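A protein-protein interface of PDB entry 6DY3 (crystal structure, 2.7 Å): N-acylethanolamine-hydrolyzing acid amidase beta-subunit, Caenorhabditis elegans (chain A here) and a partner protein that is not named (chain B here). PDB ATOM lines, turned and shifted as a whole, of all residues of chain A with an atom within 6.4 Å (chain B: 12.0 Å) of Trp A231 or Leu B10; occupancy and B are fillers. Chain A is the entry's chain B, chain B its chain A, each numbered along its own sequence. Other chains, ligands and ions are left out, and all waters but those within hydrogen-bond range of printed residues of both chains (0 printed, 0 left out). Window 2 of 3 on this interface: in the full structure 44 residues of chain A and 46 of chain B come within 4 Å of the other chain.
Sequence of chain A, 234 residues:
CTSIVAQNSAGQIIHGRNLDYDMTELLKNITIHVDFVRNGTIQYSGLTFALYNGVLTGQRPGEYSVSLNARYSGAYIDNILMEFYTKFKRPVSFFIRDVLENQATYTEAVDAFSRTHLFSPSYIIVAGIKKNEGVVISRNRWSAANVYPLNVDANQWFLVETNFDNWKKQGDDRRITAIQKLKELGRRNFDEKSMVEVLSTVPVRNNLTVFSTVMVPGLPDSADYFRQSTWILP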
ATOM      1  N   SER A 200      23.546  24.946  11.154  1.00  0.00           N
ATOM      2  CA  SER A 200      23.192  24.974  12.569  1.00  0.00           C
ATOM      3  C   SER A 200      22.795  26.360  13.060  1.00  0.00           C
ATOM      4  O   SER A 200      22.412  26.497  14.226  1.00  0.00           O
ATOM      5  CB  SER A 200      24.352  24.450  13.415  1.00  0.00           C
ATOM      6  OG  SER A 200      24.678  23.124  13.049  1.00  0.00           O
ATOM      7  N   VAL A 210      14.164  18.323  11.276  1.00  0.00           N
ATOM      8  CA  VAL A 210      14.303  16.916  11.644  1.00  0.00           C
ATOM      9  C   VAL A 210      15.770  16.512  11.666  1.00  0.00           C
ATOM     10  O   VAL A 210      16.278  15.996  12.669  1.00  0.00           O
ATOM     11  CB  VAL A 210      13.490  16.023  10.687  1.00  0.00           C
ATOM     12  CG1 VAL A 210      13.777  14.539  10.948  1.00  0.00           C
ATOM     13  CG2 VAL A 210      12.016  16.307  10.842  1.00  0.00           C
ATOM     14  N   PHE A 211      16.468  16.721  10.551  1.00  0.00           N
ATOM     15  CA  PHE A 211      17.881  16.392  10.477  1.00  0.00           C
ATOM     16  C   PHE A 211      18.628  17.447   9.680  1.00  0.00           C
ATOM     17  O   PHE A 211      18.048  18.209   8.904  1.00  0.00           O
ATOM     18  CB  PHE A 211      18.128  15.007   9.854  1.00  0.00           C
ATOM     19  CG  PHE A 211      17.700  14.884   8.411  1.00  0.00           C
ATOM     20  CD1 PHE A 211      18.459  15.436   7.393  1.00  0.00           C
ATOM     21  CD2 PHE A 211      16.577  14.152   8.076  1.00  0.00           C
ATOM     22  CE1 PHE A 211      18.076  15.304   6.080  1.00  0.00           C
ATOM     23  CE2 PHE A 211      16.195  14.010   6.758  1.00  0.00           C
ATOM     24  CZ  PHE A 211      16.944  14.583   5.761  1.00  0.00           C
ATOM     25  N   SER A 212      19.939  17.461   9.885  1.00  0.00           N
ATOM     26  CA  SER A 212      20.881  18.237   9.094  1.00  0.00           C
ATOM     27  C   SER A 212      21.905  17.267   8.523  1.00  0.00           C
ATOM     28  O   SER A 212      22.348  16.353   9.223  1.00  0.00           O
ATOM     29  CB  SER A 212      21.589  19.305   9.938  1.00  0.00           C
ATOM     30  OG  SER A 212      20.696  20.273  10.447  1.00  0.00           O
ATOM     31  N   THR A 213      22.282  17.462   7.258  1.00  0.00           N
ATOM     32  CA  THR A 213      23.212  16.562   6.595  1.00  0.00           C
ATOM     33  C   THR A 213      24.146  17.356   5.695  1.00  0.00           C
ATOM     34  O   THR A 213      23.828  18.458   5.241  1.00  0.00           O
ATOM     35  CB  THR A 213      22.476  15.484   5.780  1.00  0.00           C
ATOM     36  OG1 THR A 213      23.404  14.485   5.340  1.00  0.00           O
ATOM     37  CG2 THR A 213      21.789  16.087   4.578  1.00  0.00           C
ATOM     38  N   GLN A 228      28.024   9.078   8.005  1.00  0.00           N
ATOM     39  CA  GLN A 228      28.201   9.563   9.368  1.00  0.00           C
ATOM     40  C   GLN A 228      28.013  11.071   9.490  1.00  0.00           C
ATOM     41  O   GLN A 228      28.237  11.621  10.574  1.00  0.00           O
ATOM     42  CB  GLN A 228      29.590   9.175   9.890  1.00  0.00           C
ATOM     43  CG  GLN A 228      30.746   9.693   9.035  1.00  0.00           C
ATOM     44  CD  GLN A 228      31.096  11.145   9.306  1.00  0.00           C
ATOM     45  OE1 GLN A 228      31.470  11.514  10.421  1.00  0.00           O
ATOM     46  NE2 GLN A 228      30.953  11.983   8.286  1.00  0.00           N
ATOM     47  N   SER A 229      27.615  11.753   8.413  1.00  0.00           N
ATOM     48  CA  SER A 229      27.515  13.207   8.402  1.00  0.00           C
ATOM     49  C   SER A 229      26.135  13.734   8.793  1.00  0.00           C
ATOM     50  O   SER A 229      25.976  14.949   8.948  1.00  0.00           O
ATOM     51  CB  SER A 229      27.885  13.738   7.014  1.00  0.00           C
ATOM     52  OG  SER A 229      26.950  13.302   6.047  1.00  0.00           O
ATOM     53  N   THR A 230      25.136  12.875   8.950  1.00  0.00           N
ATOM     54  CA  THR A 230      23.791  13.338   9.257  1.00  0.00           C
ATOM     55  C   THR A 230      23.573  13.423  10.758  1.00  0.00           C
ATOM     56  O   THR A 230      24.065  12.591  11.523  1.00  0.00           O
ATOM     57  CB  THR A 230      22.746  12.419   8.634  1.00  0.00           C
ATOM     58  OG1 THR A 230      22.998  12.319   7.231  1.00  0.00           O
ATOM     59  CG2 THR A 230      21.348  12.965   8.849  1.00  0.00           C
ATOM     60  N   TRP A 231      22.800  14.426  11.164  1.00  0.00           N
ATOM     61  CA  TRP A 231      22.566  14.748  12.564  1.00  0.00           C
ATOM     62  C   TRP A 231      21.068  14.881  12.776  1.00  0.00           C
ATOM     63  O   TRP A 231      20.430  15.756  12.182  1.00  0.00           O
ATOM     64  CB  TRP A 231      23.292  16.043  12.935  1.00  0.00           C
ATOM     65  CG  TRP A 231      23.078  16.531  14.330  1.00  0.00           C
ATOM     66  CD1 TRP A 231      22.297  17.578  14.715  1.00  0.00           C
ATOM     67  CD2 TRP A 231      23.673  16.012  15.531  1.00  0.00           C
ATOM     68  NE1 TRP A 231      22.360  17.743  16.082  1.00  0.00           N
ATOM     69  CE2 TRP A 231      23.198  16.793  16.604  1.00  0.00           C
ATOM     70  CE3 TRP A 231      24.557  14.959  15.803  1.00  0.00           C
ATOM     71  CZ2 TRP A 231      23.573  16.556  17.923  1.00  0.00           C
ATOM     72  CZ3 TRP A 231      24.926  14.727  17.113  1.00  0.00           C
ATOM     73  CH2 TRP A 231      24.436  15.520  18.156  1.00  0.00           C
ATOM     74  N   ILE A 232      20.502  14.005  13.594  1.00  0.00           N
ATOM     75  CA  ILE A 232      19.098  14.106  13.968  1.00  0.00           C
ATOM     76  C   ILE A 232      19.007  15.056  15.155  1.00  0.00           C
ATOM     77  O   ILE A 232      19.608  14.809  16.207  1.00  0.00           O
ATOM     78  CB  ILE A 232      18.511  12.729  14.303  1.00  0.00           C
ATOM     79  CG1 ILE A 232      18.659  11.804  13.096  1.00  0.00           C
ATOM     80  CG2 ILE A 232      17.043  12.868  14.715  1.00  0.00           C
ATOM     81  CD1 ILE A 232      18.202  10.397  13.340  1.00  0.00           C
ATOM     82  N   LEU A 233      18.263  16.148  14.988  1.00  0.00           N
ATOM     83  CA  LEU A 233      18.346  17.199  15.988  1.00  0.00           C
ATOM     84  C   LEU A 233      17.524  16.854  17.229  1.00  0.00           C
ATOM     85  O   LEU A 233      16.471  16.223  17.128  1.00  0.00           O
ATOM     86  CB  LEU A 233      17.873  18.523  15.408  1.00  0.00           C
ATOM     87  CG  LEU A 233      18.919  19.112  14.459  1.00  0.00           C
ATOM     88  CD1 LEU A 233      18.622  18.679  13.044  1.00  0.00           C
ATOM     89  CD2 LEU A 233      19.010  20.610  14.559  1.00  0.00           C
ATOM     90  N   PRO A 234      17.987  17.265  18.419  1.00  0.00           N
ATOM     91  CA  PRO A 234      17.228  17.051  19.656  1.00  0.00           C
ATOM     92  C   PRO A 234      15.961  17.900  19.715  1.00  0.00           C
ATOM     93  O   PRO A 234      15.914  19.001  19.159  1.00  0.00           O
ATOM     94  CB  PRO A 234      18.221  17.456  20.751  1.00  0.00           C
ATOM     95  CG  PRO A 234      19.150  18.399  20.087  1.00  0.00           C
ATOM     96  CD  PRO A 234      19.285  17.913  18.682  1.00  0.00           C
ATOM     97  OXT PRO A 234      14.958  17.498  20.315  1.00  0.00           O
ATOM     98  N   LYS B   9      21.710  11.006  22.702  1.00  0.00           N
ATOM     99  CA  LYS B   9      22.084  12.331  23.192  1.00  0.00           C
ATOM    100  C   LYS B   9      23.283  12.899  22.431  1.00  0.00           C
ATOM    101  O   LYS B   9      23.178  13.935  21.772  1.00  0.00           O
ATOM    102  CB  LYS B   9      22.404  12.285  24.692  1.00  0.00           C
ATOM    103  CG  LYS B   9      22.970  13.592  25.255  1.00  0.00           C
ATOM    104  CD  LYS B   9      23.375  13.448  26.709  1.00  0.00           C
ATOM    105  CE  LYS B   9      22.187  13.496  27.641  1.00  0.00           C
ATOM    106  NZ  LYS B   9      22.614  13.435  29.066  1.00  0.00           N
ATOM    107  N   LEU B  10      24.429  12.230  22.542  1.00  0.00           N
ATOM    108  CA  LEU B  10      25.656  12.743  21.945  1.00  0.00           C
ATOM    109  C   LEU B  10      25.919  12.191  20.555  1.00  0.00           C
ATOM    110  O   LEU B  10      26.577  12.861  19.751  1.00  0.00           O
ATOM    111  CB  LEU B  10      26.853  12.430  22.846  1.00  0.00           C
ATOM    112  CG  LEU B  10      27.450  13.639  23.562  1.00  0.00           C
ATOM    113  CD1 LEU B  10      28.544  13.195  24.496  1.00  0.00           C
ATOM    114  CD2 LEU B  10      27.984  14.660  22.564  1.00  0.00           C
ATOM    115  N   ASP B  11      25.443  10.986  20.260  1.00  0.00           N
ATOM    116  CA  ASP B  11      25.519  10.406  18.922  1.00  0.00           C
ATOM    117  C   ASP B  11      24.092  10.326  18.389  1.00  0.00           C
ATOM    118  O   ASP B  11      23.358   9.377  18.684  1.00  0.00           O
ATOM    119  CB  ASP B  11      26.195   9.040  18.943  1.00  0.00           C
ATOM    120  CG  ASP B  11      27.702   9.142  19.052  1.00  0.00           C
ATOM    121  OD1 ASP B  11      28.345   9.480  18.035  1.00  0.00           O
ATOM    122  OD2 ASP B  11      28.244   8.878  20.148  1.00  0.00           O
ATOM    123  N   ARG B  12      23.704  11.330  17.614  1.00  0.00           N
ATOM    124  CA  ARG B  12      22.353  11.446  17.084  1.00  0.00           C
ATOM    125  C   ARG B  12      22.338  11.244  15.572  1.00  0.00           C
ATOM    126  O   ARG B  12      21.669  11.972  14.839  1.00  0.00           O
ATOM    127  CB  ARG B  12      21.749  12.796  17.461  1.00  0.00           C
ATOM    128  CG  ARG B  12      21.752  13.056  18.967  1.00  0.00           C
ATOM    129  CD  ARG B  12      20.920  14.270  19.351  1.00  0.00           C
ATOM    130  NE  ARG B  12      19.549  14.164  18.864  1.00  0.00           N
ATOM    131  CZ  ARG B  12      18.607  13.419  19.431  1.00  0.00           C
ATOM    132  NH1 ARG B  12      18.882  12.705  20.518  1.00  0.00           N
ATOM    133  NH2 ARG B  12      17.388  13.386  18.909  1.00  0.00           N
ATOM    134  N   LYS B  13      23.093  10.245  15.091  1.00  0.00           N
ATOM    135  CA  LYS B  13      23.118   9.899  13.681  1.00  0.00           C
ATOM    136  C   LYS B  13      21.989   8.928  13.356  1.00  0.00           C
ATOM    137  O   LYS B  13      21.594   8.122  14.205  1.00  0.00           O
ATOM    138  CB  LYS B  13      24.453   9.252  13.306  1.00  0.00           C
ATOM    139  CG  LYS B  13      25.666  10.148  13.501  1.00  0.00           C
ATOM    140  CD  LYS B  13      26.953   9.382  13.291  1.00  0.00           C
ATOM    141  CE  LYS B  13      28.168  10.238  13.622  1.00  0.00           C
ATOM    142  NZ  LYS B  13      29.439   9.456  13.586  1.00  0.00           N
ATOM    143  N   PRO B  14      21.458   8.982  12.137  1.00  0.00           N
ATOM    144  CA  PRO B  14      20.434   8.006  11.746  1.00  0.00           C
ATOM    145  C   PRO B  14      21.033   6.620  11.571  1.00  0.00           C
ATOM    146  O   PRO B  14      22.165   6.467  11.107  1.00  0.00           O
ATOM    147  CB  PRO B  14      19.907   8.558  10.417  1.00  0.00           C
ATOM    148  CG  PRO B  14      21.021   9.372   9.880  1.00  0.00           C
ATOM    149  CD  PRO B  14      21.708   9.970  11.075  1.00  0.00           C
ATOM    150  N   ARG B  15      20.254   5.606  11.944  1.00  0.00           N
ATOM    151  CA  ARG B  15      20.698   4.227  11.796  1.00  0.00           C
ATOM    152  C   ARG B  15      20.972   3.907  10.331  1.00  0.00           C
ATOM    153  O   ARG B  15      20.211   4.297   9.441  1.00  0.00           O
ATOM    154  CB  ARG B  15      19.649   3.262  12.346  1.00  0.00           C
ATOM    155  CG  ARG B  15      19.518   3.273  13.863  1.00  0.00           C
ATOM    156  CD  ARG B  15      18.731   2.065  14.349  1.00  0.00           C
ATOM    157  NE  ARG B  15      19.347   0.811  13.916  1.00  0.00           N
ATOM    158  CZ  ARG B  15      18.907  -0.399  14.248  1.00  0.00           C
ATOM    159  NH1 ARG B  15      17.837  -0.531  15.025  1.00  0.00           N
ATOM    160  NH2 ARG B  15      19.542  -1.480  13.804  1.00  0.00           N
ATOM    161  N   HIS B  16      22.057   3.181  10.084  1.00  0.00           N
ATOM    162  CA  HIS B  16      22.475   2.860   8.728  1.00  0.00           C
ATOM    163  C   HIS B  16      22.002   1.466   8.344  1.00  0.00           C
ATOM    164  O   HIS B  16      22.071   0.532   9.148  1.00  0.00           O
ATOM    165  CB  HIS B  16      23.993   2.944   8.581  1.00  0.00           C
ATOM    166  CG  HIS B  16      24.499   2.369   7.298  1.00  0.00           C
ATOM    167  ND1 HIS B  16      25.314   1.258   7.250  1.00  0.00           N
ATOM    168  CD2 HIS B  16      24.294   2.740   6.013  1.00  0.00           C
ATOM    169  CE1 HIS B  16      25.599   0.979   5.991  1.00  0.00           C
ATOM    170  NE2 HIS B  16      24.991   1.863   5.220  1.00  0.00           N
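O of Arg B12 lies within hydrogen-bond range of N of Ile A232.
The guanidinium group of Arg B12 is in hydrogen-bond range of the backbone carbonyl oxygen of Leu A233.
The backbone carbonyl oxygen of Ser A212 sits at hydrogen-bond distance from the backbone NH of Trp A231, at 2.8 Å.
N of Leu A233 is in hydrogen-bond range of O of Val A210, 3.1 Å away.
The side-chain hydroxyl of Thr A230 lies within hydrogen-bond range of the side-chain hydroxyl of Thr A213, 2.9 Å away.
Among the printed residues, pairs that only touch across the chains: Gln A228 with Lys B13 (3.3 Å), Pro A234 with Arg B12 (3.5 Å), Thr A230 with Lys B13 (3.5 Å), Thr A230 with Pro B14 (3.6 Å), Trp A231 with Arg B12 (3.6 Å), Trp A231 with Leu B10 (3.6 Å) and Ile A232 with Pro B14 (3.6 Å).
Trp A231 touches just these residues of chain B: Leu B10 (3.6 Å) and Arg B12 (3.6 Å).
Of chain A, only Trp A231 comes within 4 Å of Leu B10.
No residue of chain B comes within 4 Å of Phe A211.
No residue of chain B comes within 4 Å of Ser A229.
Ile A232 touches just these residues of chain B: Arg B12 (2.7 Å) and Pro B14 (3.6 Å).
Of chain B, only Arg B12 comes within 4 Å of Leu A233.
Printed residues of chain A within 4 Å of Arg B12: Trp A231 (3.6 Å), Ile A232 (2.7 Å), Leu A233 (3.5 Å) and Pro A234 (3.5 Å).
Of the printed residues of chain A, Lys B13 touches Gln A228 and Thr A230.
Of the printed residues of chain B, Gln A228 touches Lys B13.
Of the printed residues of chain A, Pro B14 touches Thr A230 (3.6 Å) and Ile A232 (3.6 Å).
Of the printed residues of chain B, Pro A234 touches Arg B12 (3.5 Å).
The nearest residue of chain B that does not touch Trp A231 is Lys B9 (4.1 Å).
The nearest printed residue of chain B that does not touch Pro A234 is Lys B9 (6.2 Å).
Hydrophobic or aromatic side chains of chain A that line the printed part of chain B: Trp A231, Ile A232 and Pro A234.
Printed residues of chain B that touch a printed residue of chain A: Leu B10, Arg B12, Lys B13 and Pro B14.
Among the printed residues, 9 pairs touch across the chains.
Among the printed residues, no Asp or Glu carboxylate lies within 4 Å of a Lys or Arg side-chain nitrogen of the other chain.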
